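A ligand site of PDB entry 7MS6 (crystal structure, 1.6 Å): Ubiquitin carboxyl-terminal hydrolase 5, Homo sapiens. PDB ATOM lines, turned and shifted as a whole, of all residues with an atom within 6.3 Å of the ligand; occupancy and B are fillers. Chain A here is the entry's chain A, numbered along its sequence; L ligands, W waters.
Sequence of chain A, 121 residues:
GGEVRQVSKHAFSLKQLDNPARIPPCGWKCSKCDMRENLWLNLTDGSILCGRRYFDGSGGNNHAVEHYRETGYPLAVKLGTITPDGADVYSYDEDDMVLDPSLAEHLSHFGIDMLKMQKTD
O1 of the ligand is in hydrogen-bond range of OH of Tyr 92, 2.7 Å away.
The backbone NH (N) of Arg 52 sits at hydrogen-bond distance from an oxygen (O5) of the ligand (2.9 Å).
NH2 of Arg 52 sits at hydrogen-bond distance from O2 of the ligand (2.9 Å).
OH of Tyr 90 lies within hydrogen-bond range of OD1 of Asp 95 (3.0 Å).
N of Trp 40 is in hydrogen-bond range of O of Leu 49, 2.8 Å away.
N of Tyr 90 sits at hydrogen-bond distance from O of Ala 76, at 2.8 Å.
The backbone carbonyl oxygen (O) of Gly 51 sits at hydrogen-bond distance from the backbone NH (N) of Asn 62 (3.1 Å).
The side-chain carboxylate (OD1) of Asp 56 is in hydrogen-bond range of the side-chain hydroxyl (OG) of Ser 58 (2.7 Å).
O of Asn 38 is in hydrogen-bond range of N of Gly 51.
The backbone carbonyl oxygen (O) of Cys 50 lies within hydrogen-bond range of the backbone NH (N) of Ala 64.
NE1 of Trp 40 sits at hydrogen-bond distance from OD1 of Asn 38 (3.0 Å).
A fluorine (F1) of the ligand sits close to the side-chain sulfur of Met 97, 3.6 Å away.
Merely in contact with the ligand: Trp 40, Gly 51, Tyr 54, Phe 55, Asp 56, Ser 58, Ala 64, Val 65 and Tyr 90.
Hydrophobic or aromatic side chains within 4 Å of the ligand: Trp 40, Tyr 54, Phe 55, Ala 64, Tyr 90, Tyr 92 and Met 97.
Within 4 Å of the ligand: Trp 40, Gly 51, Arg 52, Tyr 54, Phe 55, Asp 56, Ser 58, Ala 64, Val 65, Tyr 90, Tyr 92 and Met 97.
The nearest printed residue that does not touch the ligand is Cys 50 (4.4 Å).
Water W1 lies within hydrogen-bond range of an oxygen (O5) of the ligand (2.7 Å) and the side-chain hydroxyl (OH) of Tyr 54 (2.8 Å).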
ATOM      1  N   ARG A   5      18.274 -18.016  -7.043  1.00  0.00           N
ATOM      2  CA  ARG A   5      16.947 -17.358  -6.957  1.00  0.00           C
ATOM      3  C   ARG A   5      16.578 -16.819  -8.343  1.00  0.00           C
ATOM      4  O   ARG A   5      17.485 -16.312  -9.056  1.00  0.00           O
ATOM      5  CB  ARG A   5      16.956 -16.238  -5.907  1.00  0.00           C
ATOM      6  CG  ARG A   5      16.959 -16.794  -4.507  1.00  0.00           C
ATOM      7  CD  ARG A   5      17.106 -15.729  -3.455  1.00  0.00           C
ATOM      8  NE  ARG A   5      17.384 -16.365  -2.182  1.00  0.00           N
ATOM      9  CZ  ARG A   5      17.738 -15.750  -1.074  1.00  0.00           C
ATOM     10  NH1 ARG A   5      17.712 -14.442  -1.022  1.00  0.00           N
ATOM     11  NH2 ARG A   5      18.058 -16.441   0.011  1.00  0.00           N
ATOM     12  N   ASN A  38      13.436  -9.621  12.252  1.00  0.00           N
ATOM     13  CA  ASN A  38      12.656 -10.370  11.257  1.00  0.00           C
ATOM     14  C   ASN A  38      11.488  -9.535  10.782  1.00  0.00           C
ATOM     15  O   ASN A  38      10.329  -9.987  10.761  1.00  0.00           O
ATOM     16  CB  ASN A  38      12.166 -11.687  11.831  1.00  0.00           C
ATOM     17  CG  ASN A  38      11.582 -12.632  10.818  1.00  0.00           C
ATOM     18  OD1 ASN A  38      11.829 -12.555   9.635  1.00  0.00           O
ATOM     19  ND2 ASN A  38      10.783 -13.549  11.332  1.00  0.00           N
ATOM     20  N   TRP A  40       9.825  -7.161   7.609  1.00  0.00           N
ATOM     21  CA  TRP A  40       9.705  -7.215   6.139  1.00  0.00           C
ATOM     22  C   TRP A  40       9.035  -5.936   5.696  1.00  0.00           C
ATOM     23  O   TRP A  40       7.924  -5.609   6.148  1.00  0.00           O
ATOM     24  CB  TRP A  40       8.961  -8.457   5.718  1.00  0.00           C
ATOM     25  CG  TRP A  40       9.722  -9.707   6.060  1.00  0.00           C
ATOM     26  CD1 TRP A  40       9.830 -10.317   7.280  1.00  0.00           C
ATOM     27  CD2 TRP A  40      10.520 -10.463   5.148  1.00  0.00           C
ATOM     28  NE1 TRP A  40      10.648 -11.399   7.169  1.00  0.00           N
ATOM     29  CE2 TRP A  40      11.059 -11.536   5.873  1.00  0.00           C
ATOM     30  CE3 TRP A  40      10.764 -10.393   3.776  1.00  0.00           C
ATOM     31  CZ2 TRP A  40      11.865 -12.506   5.283  1.00  0.00           C
ATOM     32  CZ3 TRP A  40      11.592 -11.349   3.221  1.00  0.00           C
ATOM     33  CH2 TRP A  40      12.096 -12.408   3.945  1.00  0.00           C
ATOM     34  N   LEU A  49       6.406  -5.052   8.759  1.00  0.00           N
ATOM     35  CA  LEU A  49       5.594  -6.074   9.456  1.00  0.00           C
ATOM     36  C   LEU A  49       6.422  -7.323   9.618  1.00  0.00           C
ATOM     37  O   LEU A  49       7.316  -7.608   8.781  1.00  0.00           O
ATOM     38  CB  LEU A  49       4.319  -6.354   8.678  1.00  0.00           C
ATOM     39  CG  LEU A  49       3.382  -5.154   8.540  1.00  0.00           C
ATOM     40  CD1 LEU A  49       2.343  -5.423   7.470  1.00  0.00           C
ATOM     41  CD2 LEU A  49       2.712  -4.749   9.863  1.00  0.00           C
ATOM     42  N   CYS A  50       6.193  -8.092  10.694  1.00  0.00           N
ATOM     43  CA  CYS A  50       7.044  -9.232  11.032  1.00  0.00           C
ATOM     44  C   CYS A  50       6.818 -10.447  10.131  1.00  0.00           C
ATOM     45  O   CYS A  50       5.758 -10.662   9.538  1.00  0.00           O
ATOM     46  CB  CYS A  50       6.828  -9.585  12.503  1.00  0.00           C
ATOM     47  SG  CYS A  50       5.133 -10.102  12.899  1.00  0.00           S
ATOM     48  N   GLY A  51       7.860 -11.277  10.132  1.00  0.00           N
ATOM     49  CA  GLY A  51       7.862 -12.493   9.322  1.00  0.00           C
ATOM     50  C   GLY A  51       6.967 -13.611   9.865  1.00  0.00           C
ATOM     51  O   GLY A  51       6.406 -13.513  10.985  1.00  0.00           O
ATOM     52  N   ARG A  52       6.805 -14.653   9.057  1.00  0.00           N
ATOM     53  CA  ARG A  52       5.811 -15.683   9.362  1.00  0.00           C
ATOM     54  C   ARG A  52       6.379 -16.626  10.446  1.00  0.00           C
ATOM     55  O   ARG A  52       7.574 -16.728  10.668  1.00  0.00           O
ATOM     56  CB  ARG A  52       5.376 -16.402   8.071  1.00  0.00           C
ATOM     57  CG  ARG A  52       6.264 -17.524   7.604  1.00  0.00           C
ATOM     58  CD  ARG A  52       5.537 -18.269   6.462  1.00  0.00           C
ATOM     59  NE  ARG A  52       5.527 -17.453   5.301  1.00  0.00           N
ATOM     60  CZ  ARG A  52       4.621 -17.431   4.360  1.00  0.00           C
ATOM     61  NH1 ARG A  52       3.472 -18.093   4.451  1.00  0.00           N
ATOM     62  NH2 ARG A  52       4.864 -16.699   3.293  1.00  0.00           N
ATOM     63  N   ARG A  53       5.443 -17.301  11.089  1.00  0.00           N
ATOM     64  CA  ARG A  53       5.718 -18.370  12.078  1.00  0.00           C
ATOM     65  C   ARG A  53       5.811 -19.705  11.380  1.00  0.00           C
ATOM     66  O   ARG A  53       4.981 -20.025  10.518  1.00  0.00           O
ATOM     67  CB  ARG A  53       4.577 -18.417  13.079  1.00  0.00           C
ATOM     68  CG  ARG A  53       4.866 -19.276  14.282  1.00  0.00           C
ATOM     69  CD  ARG A  53       5.985 -18.862  15.223  1.00  0.00           C
ATOM     70  NE  ARG A  53       5.768 -17.509  15.740  1.00  0.00           N
ATOM     71  CZ  ARG A  53       6.365 -17.021  16.821  1.00  0.00           C
ATOM     72  NH1 ARG A  53       6.053 -15.786  17.217  1.00  0.00           N
ATOM     73  NH2 ARG A  53       7.191 -17.770  17.509  1.00  0.00           N
ATOM     74  N   TYR A  54       6.812 -20.473  11.773  1.00  0.00           N
ATOM     75  CA  TYR A  54       7.022 -21.834  11.254  1.00  0.00           C
ATOM     76  C   TYR A  54       6.634 -22.905  12.283  1.00  0.00           C
ATOM     77  O   TYR A  54       6.465 -22.639  13.488  1.00  0.00           O
ATOM     78  CB  TYR A  54       8.461 -21.988  10.733  1.00  0.00           C
ATOM     79  CG  TYR A  54       8.737 -21.113   9.533  1.00  0.00           C
ATOM     80  CD1 TYR A  54       8.327 -21.527   8.280  1.00  0.00           C
ATOM     81  CD2 TYR A  54       9.325 -19.885   9.684  1.00  0.00           C
ATOM     82  CE1 TYR A  54       8.510 -20.701   7.159  1.00  0.00           C
ATOM     83  CE2 TYR A  54       9.543 -19.078   8.585  1.00  0.00           C
ATOM     84  CZ  TYR A  54       9.154 -19.498   7.344  1.00  0.00           C
ATOM     85  OH  TYR A  54       9.314 -18.671   6.246  1.00  0.00           O
ATOM     86  N   PHE A  55       6.562 -24.149  11.803  1.00  0.00           N
ATOM     87  CA  PHE A  55       6.091 -25.308  12.583  1.00  0.00           C
ATOM     88  C   PHE A  55       6.942 -25.522  13.839  1.00  0.00           C
ATOM     89  O   PHE A  55       6.406 -26.164  14.759  1.00  0.00           O
ATOM     90  CB  PHE A  55       6.171 -26.582  11.701  1.00  0.00           C
ATOM     91  CG  PHE A  55       7.600 -26.936  11.381  1.00  0.00           C
ATOM     92  CD1 PHE A  55       8.256 -26.293  10.330  1.00  0.00           C
ATOM     93  CD2 PHE A  55       8.278 -27.858  12.152  1.00  0.00           C
ATOM     94  CE1 PHE A  55       9.606 -26.558  10.110  1.00  0.00           C
ATOM     95  CE2 PHE A  55       9.631 -28.086  11.927  1.00  0.00           C
ATOM     96  CZ  PHE A  55      10.270 -27.440  10.922  1.00  0.00           C
ATOM     97  N   ASP A  56       8.216 -25.113  13.893  1.00  0.00           N
ATOM     98  CA  ASP A  56       9.107 -25.361  15.049  1.00  0.00           C
ATOM     99  C   ASP A  56       9.049 -24.220  16.055  1.00  0.00           C
ATOM    100  O   ASP A  56       9.782 -24.250  17.049  1.00  0.00           O
ATOM    101  CB  ASP A  56      10.523 -25.629  14.547  1.00  0.00           C
ATOM    102  CG  ASP A  56      11.172 -24.437  13.875  1.00  0.00           C
ATOM    103  OD1 ASP A  56      10.435 -23.513  13.484  1.00  0.00           O
ATOM    104  OD2 ASP A  56      12.395 -24.416  13.781  1.00  0.00           O
ATOM    105  N   SER A  58       9.884 -21.124  15.229  1.00  0.00           N
ATOM    106  CA  SER A  58      10.751 -20.042  14.715  1.00  0.00           C
ATOM    107  C   SER A  58       9.895 -19.047  13.934  1.00  0.00           C
ATOM    108  O   SER A  58       8.793 -19.372  13.472  1.00  0.00           O
ATOM    109  CB  SER A  58      11.870 -20.572  13.930  1.00  0.00           C
ATOM    110  OG  SER A  58      11.476 -21.119  12.706  1.00  0.00           O
ATOM    111  N   ASN A  62       3.443 -13.313  11.758  1.00  0.00           N
ATOM    112  CA  ASN A  62       2.697 -13.435  10.508  1.00  0.00           C
ATOM    113  C   ASN A  62       2.115 -12.101  10.029  1.00  0.00           C
ATOM    114  O   ASN A  62       1.278 -12.092   9.147  1.00  0.00           O
ATOM    115  CB  ASN A  62       1.529 -14.428  10.605  1.00  0.00           C
ATOM    116  CG  ASN A  62       1.968 -15.809  10.976  1.00  0.00           C
ATOM    117  OD1 ASN A  62       2.857 -16.381  10.375  1.00  0.00           O
ATOM    118  ND2 ASN A  62       1.333 -16.362  12.007  1.00  0.00           N
ATOM    119  N   HIS A  63       2.629 -10.967  10.523  1.00  0.00           N
ATOM    120  CA  HIS A  63       1.981  -9.708  10.157  1.00  0.00           C
ATOM    121  C   HIS A  63       2.223  -9.347   8.678  1.00  0.00           C
ATOM    122  O   HIS A  63       1.328  -8.859   8.024  1.00  0.00           O
ATOM    123  CB  HIS A  63       2.257  -8.624  11.197  1.00  0.00           C
ATOM    124  CG  HIS A  63       1.572  -8.954  12.492  1.00  0.00           C
ATOM    125  ND1 HIS A  63       2.226  -8.856  13.646  1.00  0.00           N
ATOM    126  CD2 HIS A  63       0.260  -9.304  12.714  1.00  0.00           C
ATOM    127  CE1 HIS A  63       1.331  -9.206  14.593  1.00  0.00           C
ATOM    128  NE2 HIS A  63       0.100  -9.416  14.047  1.00  0.00           N
ATOM    129  N   ALA A  64       3.396  -9.623   8.125  1.00  0.00           N
ATOM    130  CA  ALA A  64       3.665  -9.324   6.723  1.00  0.00           C
ATOM    131  C   ALA A  64       2.867 -10.198   5.777  1.00  0.00           C
ATOM    132  O   ALA A  64       2.304  -9.694   4.824  1.00  0.00           O
ATOM    133  CB  ALA A  64       5.158  -9.398   6.471  1.00  0.00           C
ATOM    134  N   VAL A  65       2.747 -11.475   6.099  1.00  0.00           N
ATOM    135  CA  VAL A  65       1.963 -12.384   5.214  1.00  0.00           C
ATOM    136  C   VAL A  65       0.482 -12.087   5.389  1.00  0.00           C
ATOM    137  O   VAL A  65      -0.250 -12.098   4.408  1.00  0.00           O
ATOM    138  CB  VAL A  65       2.313 -13.858   5.386  1.00  0.00           C
ATOM    139  CG1 VAL A  65       1.881 -14.382   6.749  1.00  0.00           C
ATOM    140  CG2 VAL A  65       1.649 -14.698   4.284  1.00  0.00           C
ATOM    141  N   ALA A  76       8.205  -8.354  -0.610  1.00  0.00           N
ATOM    142  CA  ALA A  76       8.737  -7.742   0.599  1.00  0.00           C
ATOM    143  C   ALA A  76      10.218  -8.040   0.722  1.00  0.00           C
ATOM    144  O   ALA A  76      10.682  -9.131   0.425  1.00  0.00           O
ATOM    145  CB  ALA A  76       7.943  -8.125   1.815  1.00  0.00           C
ATOM    146  N   LYS A  78      13.530  -8.165   3.430  1.00  0.00           N
ATOM    147  CA  LYS A  78      13.837  -8.359   4.856  1.00  0.00           C
ATOM    148  C   LYS A  78      14.784  -7.237   5.300  1.00  0.00           C
ATOM    149  O   LYS A  78      15.930  -7.121   4.798  1.00  0.00           O
ATOM    150  CB  LYS A  78      14.425  -9.723   5.154  1.00  0.00           C
ATOM    151  CG  LYS A  78      14.567  -9.981   6.633  1.00  0.00           C
ATOM    152  CD  LYS A  78      15.102 -11.381   6.873  1.00  0.00           C
ATOM    153  CE  LYS A  78      15.163 -11.664   8.340  1.00  0.00           C
ATOM    154  NZ  LYS A  78      15.747 -12.986   8.638  1.00  0.00           N
ATOM    155  N   TYR A  90      11.221 -11.665  -0.724  1.00  0.00           N
ATOM    156  CA  TYR A  90      10.286 -12.796  -0.867  1.00  0.00           C
ATOM    157  C   TYR A  90       9.114 -12.325  -1.711  1.00  0.00           C
ATOM    158  O   TYR A  90       8.657 -11.161  -1.599  1.00  0.00           O
ATOM    159  CB  TYR A  90       9.789 -13.272   0.504  1.00  0.00           C
ATOM    160  CG  TYR A  90       8.842 -14.452   0.451  1.00  0.00           C
ATOM    161  CD1 TYR A  90       9.340 -15.701   0.171  1.00  0.00           C
ATOM    162  CD2 TYR A  90       7.461 -14.289   0.601  1.00  0.00           C
ATOM    163  CE1 TYR A  90       8.482 -16.794   0.113  1.00  0.00           C
ATOM    164  CE2 TYR A  90       6.622 -15.369   0.592  1.00  0.00           C
ATOM    165  CZ  TYR A  90       7.123 -16.612   0.277  1.00  0.00           C
ATOM    166  OH  TYR A  90       6.278 -17.707   0.236  1.00  0.00           O
ATOM    167  N   TYR A  92       5.257 -13.294  -2.121  1.00  0.00           N
ATOM    168  CA  TYR A  92       4.123 -14.043  -1.564  1.00  0.00           C
ATOM    169  C   TYR A  92       3.304 -14.653  -2.709  1.00  0.00           C
ATOM    170  O   TYR A  92       2.749 -15.731  -2.491  1.00  0.00           O
ATOM    171  CB  TYR A  92       3.240 -13.100  -0.753  1.00  0.00           C
ATOM    172  CG  TYR A  92       3.932 -12.548   0.469  1.00  0.00           C
ATOM    173  CD1 TYR A  92       4.082 -13.288   1.607  1.00  0.00           C
ATOM    174  CD2 TYR A  92       4.427 -11.262   0.499  1.00  0.00           C
ATOM    175  CE1 TYR A  92       4.734 -12.812   2.730  1.00  0.00           C
ATOM    176  CE2 TYR A  92       5.056 -10.752   1.603  1.00  0.00           C
ATOM    177  CZ  TYR A  92       5.228 -11.545   2.737  1.00  0.00           C
ATOM    178  OH  TYR A  92       5.893 -11.002   3.793  1.00  0.00           O
ATOM    179  N   ASP A  95       5.418 -17.598  -4.131  1.00  0.00           N
ATOM    180  CA  ASP A  95       5.808 -18.584  -3.111  1.00  0.00           C
ATOM    181  C   ASP A  95       7.295 -18.870  -3.183  1.00  0.00           C
ATOM    182  O   ASP A  95       7.705 -20.060  -3.125  1.00  0.00           O
ATOM    183  CB  ASP A  95       4.967 -19.857  -3.281  1.00  0.00           C
ATOM    184  CG  ASP A  95       5.189 -20.828  -2.148  1.00  0.00           C
ATOM    185  OD1 ASP A  95       5.623 -20.388  -1.041  1.00  0.00           O
ATOM    186  OD2 ASP A  95       5.049 -22.025  -2.432  1.00  0.00           O
ATOM    187  N   ASP A  96       8.164 -17.867  -3.219  1.00  0.00           N
ATOM    188  CA  ASP A  96       9.615 -18.132  -3.262  1.00  0.00           C
ATOM    189  C   ASP A  96      10.408 -16.867  -2.937  1.00  0.00           C
ATOM    190  O   ASP A  96       9.906 -15.740  -3.150  1.00  0.00           O
ATOM    191  CB  ASP A  96      10.046 -18.551  -4.679  1.00  0.00           C
ATOM    192  CG  ASP A  96      10.184 -20.028  -4.994  1.00  0.00           C
ATOM    193  OD1 ASP A  96      10.812 -20.705  -4.234  1.00  0.00           O
ATOM    194  OD2 ASP A  96       9.694 -20.442  -6.083  1.00  0.00           O
ATOM    195  N   MET A  97      11.603 -17.055  -2.427  1.00  0.00           N
ATOM    196  CA  MET A  97      12.633 -16.015  -2.432  1.00  0.00           C
ATOM    197  C   MET A  97      12.914 -15.709  -3.911  1.00  0.00           C
ATOM    198  O   MET A  97      12.960 -16.648  -4.746  1.00  0.00           O
ATOM    199  CB  MET A  97      13.908 -16.444  -1.737  1.00  0.00           C
ATOM    200  CG  MET A  97      13.667 -16.828  -0.272  1.00  0.00           C
ATOM    201  SD  MET A  97      13.068 -15.480   0.736  1.00  0.00           S
ATOM    202  CE  MET A  97      14.430 -14.337   0.559  1.00  0.00           C
HETATM  203  C1  LIG L   1      13.251 -20.301   5.301  1.00  0.00           C
HETATM  204  C2  LIG L   1      11.310 -21.618   4.593  1.00  0.00           C
HETATM  205  C3  LIG L   1      11.642 -22.617   5.708  1.00  0.00           C
HETATM  206  C4  LIG L   1      12.295 -21.940   6.896  1.00  0.00           C
HETATM  207  C5  LIG L   1      12.584 -22.910   8.023  1.00  0.00           C
HETATM  208  C6  LIG L   1      13.544 -23.895   7.912  1.00  0.00           C
HETATM  209  C7  LIG L   1      13.057 -24.662  10.134  1.00  0.00           C
HETATM  210  C8  LIG L   1      12.080 -23.712  10.232  1.00  0.00           C
HETATM  211  C9  LIG L   1      11.838 -22.847   9.186  1.00  0.00           C
HETATM  212  C10 LIG L   1      11.520 -18.815   2.948  1.00  0.00           C
HETATM  213  C11 LIG L   1      10.163 -18.982   2.773  1.00  0.00           C
HETATM  214  C12 LIG L   1       9.308 -17.930   3.034  1.00  0.00           C
HETATM  215  C13 LIG L   1       9.813 -16.704   3.486  1.00  0.00           C
HETATM  216  C14 LIG L   1       8.775 -15.662   3.790  1.00  0.00           C
HETATM  217  C15 LIG L   1       8.231 -13.346   4.306  1.00  0.00           C
HETATM  218  C16 LIG L   1       7.434 -13.450   5.596  1.00  0.00           C
HETATM  219  C17 LIG L   1      11.177 -16.601   3.645  1.00  0.00           C
HETATM  220  C18 LIG L   1      12.077 -17.640   3.395  1.00  0.00           C
HETATM  221  O1  LIG L   1       6.401 -12.815   5.765  1.00  0.00           O
HETATM  222  O2  LIG L   1       7.578 -15.923   3.723  1.00  0.00           O
HETATM  223  O3  LIG L   1      13.872 -19.730   2.566  1.00  0.00           O
HETATM  224  O4  LIG L   1      11.887 -21.073   1.840  1.00  0.00           O
HETATM  225  S1  LIG L   1      12.569 -20.217   2.743  1.00  0.00           S
HETATM  226  F1  LIG L   1      11.716 -15.450   4.088  1.00  0.00           F
HETATM  227  N1  LIG L   1       9.190 -14.398   4.033  1.00  0.00           N
HETATM  228  O5  LIG L   1       7.913 -14.313   6.445  1.00  0.00           O
HETATM  229  N2  LIG L   1      12.565 -20.984   4.200  1.00  0.00           N
HETATM  230  C19 LIG L   1      13.554 -21.247   6.447  1.00  0.00           C
HETATM  231  C20 LIG L   1      13.772 -24.789   8.962  1.00  0.00           C
HETATM  232  O   HOH W   1       9.965 -15.998   6.861  1.00  0.00           O
HETATM  233  O   HOH W   2      12.741 -16.498   6.965  1.00  0.00           O
HETATM  234  O   HOH W   3      14.852 -16.898   5.147  1.00  0.00           O
HETATM  235  O   HOH W   4       4.676 -12.670   7.877  1.00  0.00           O
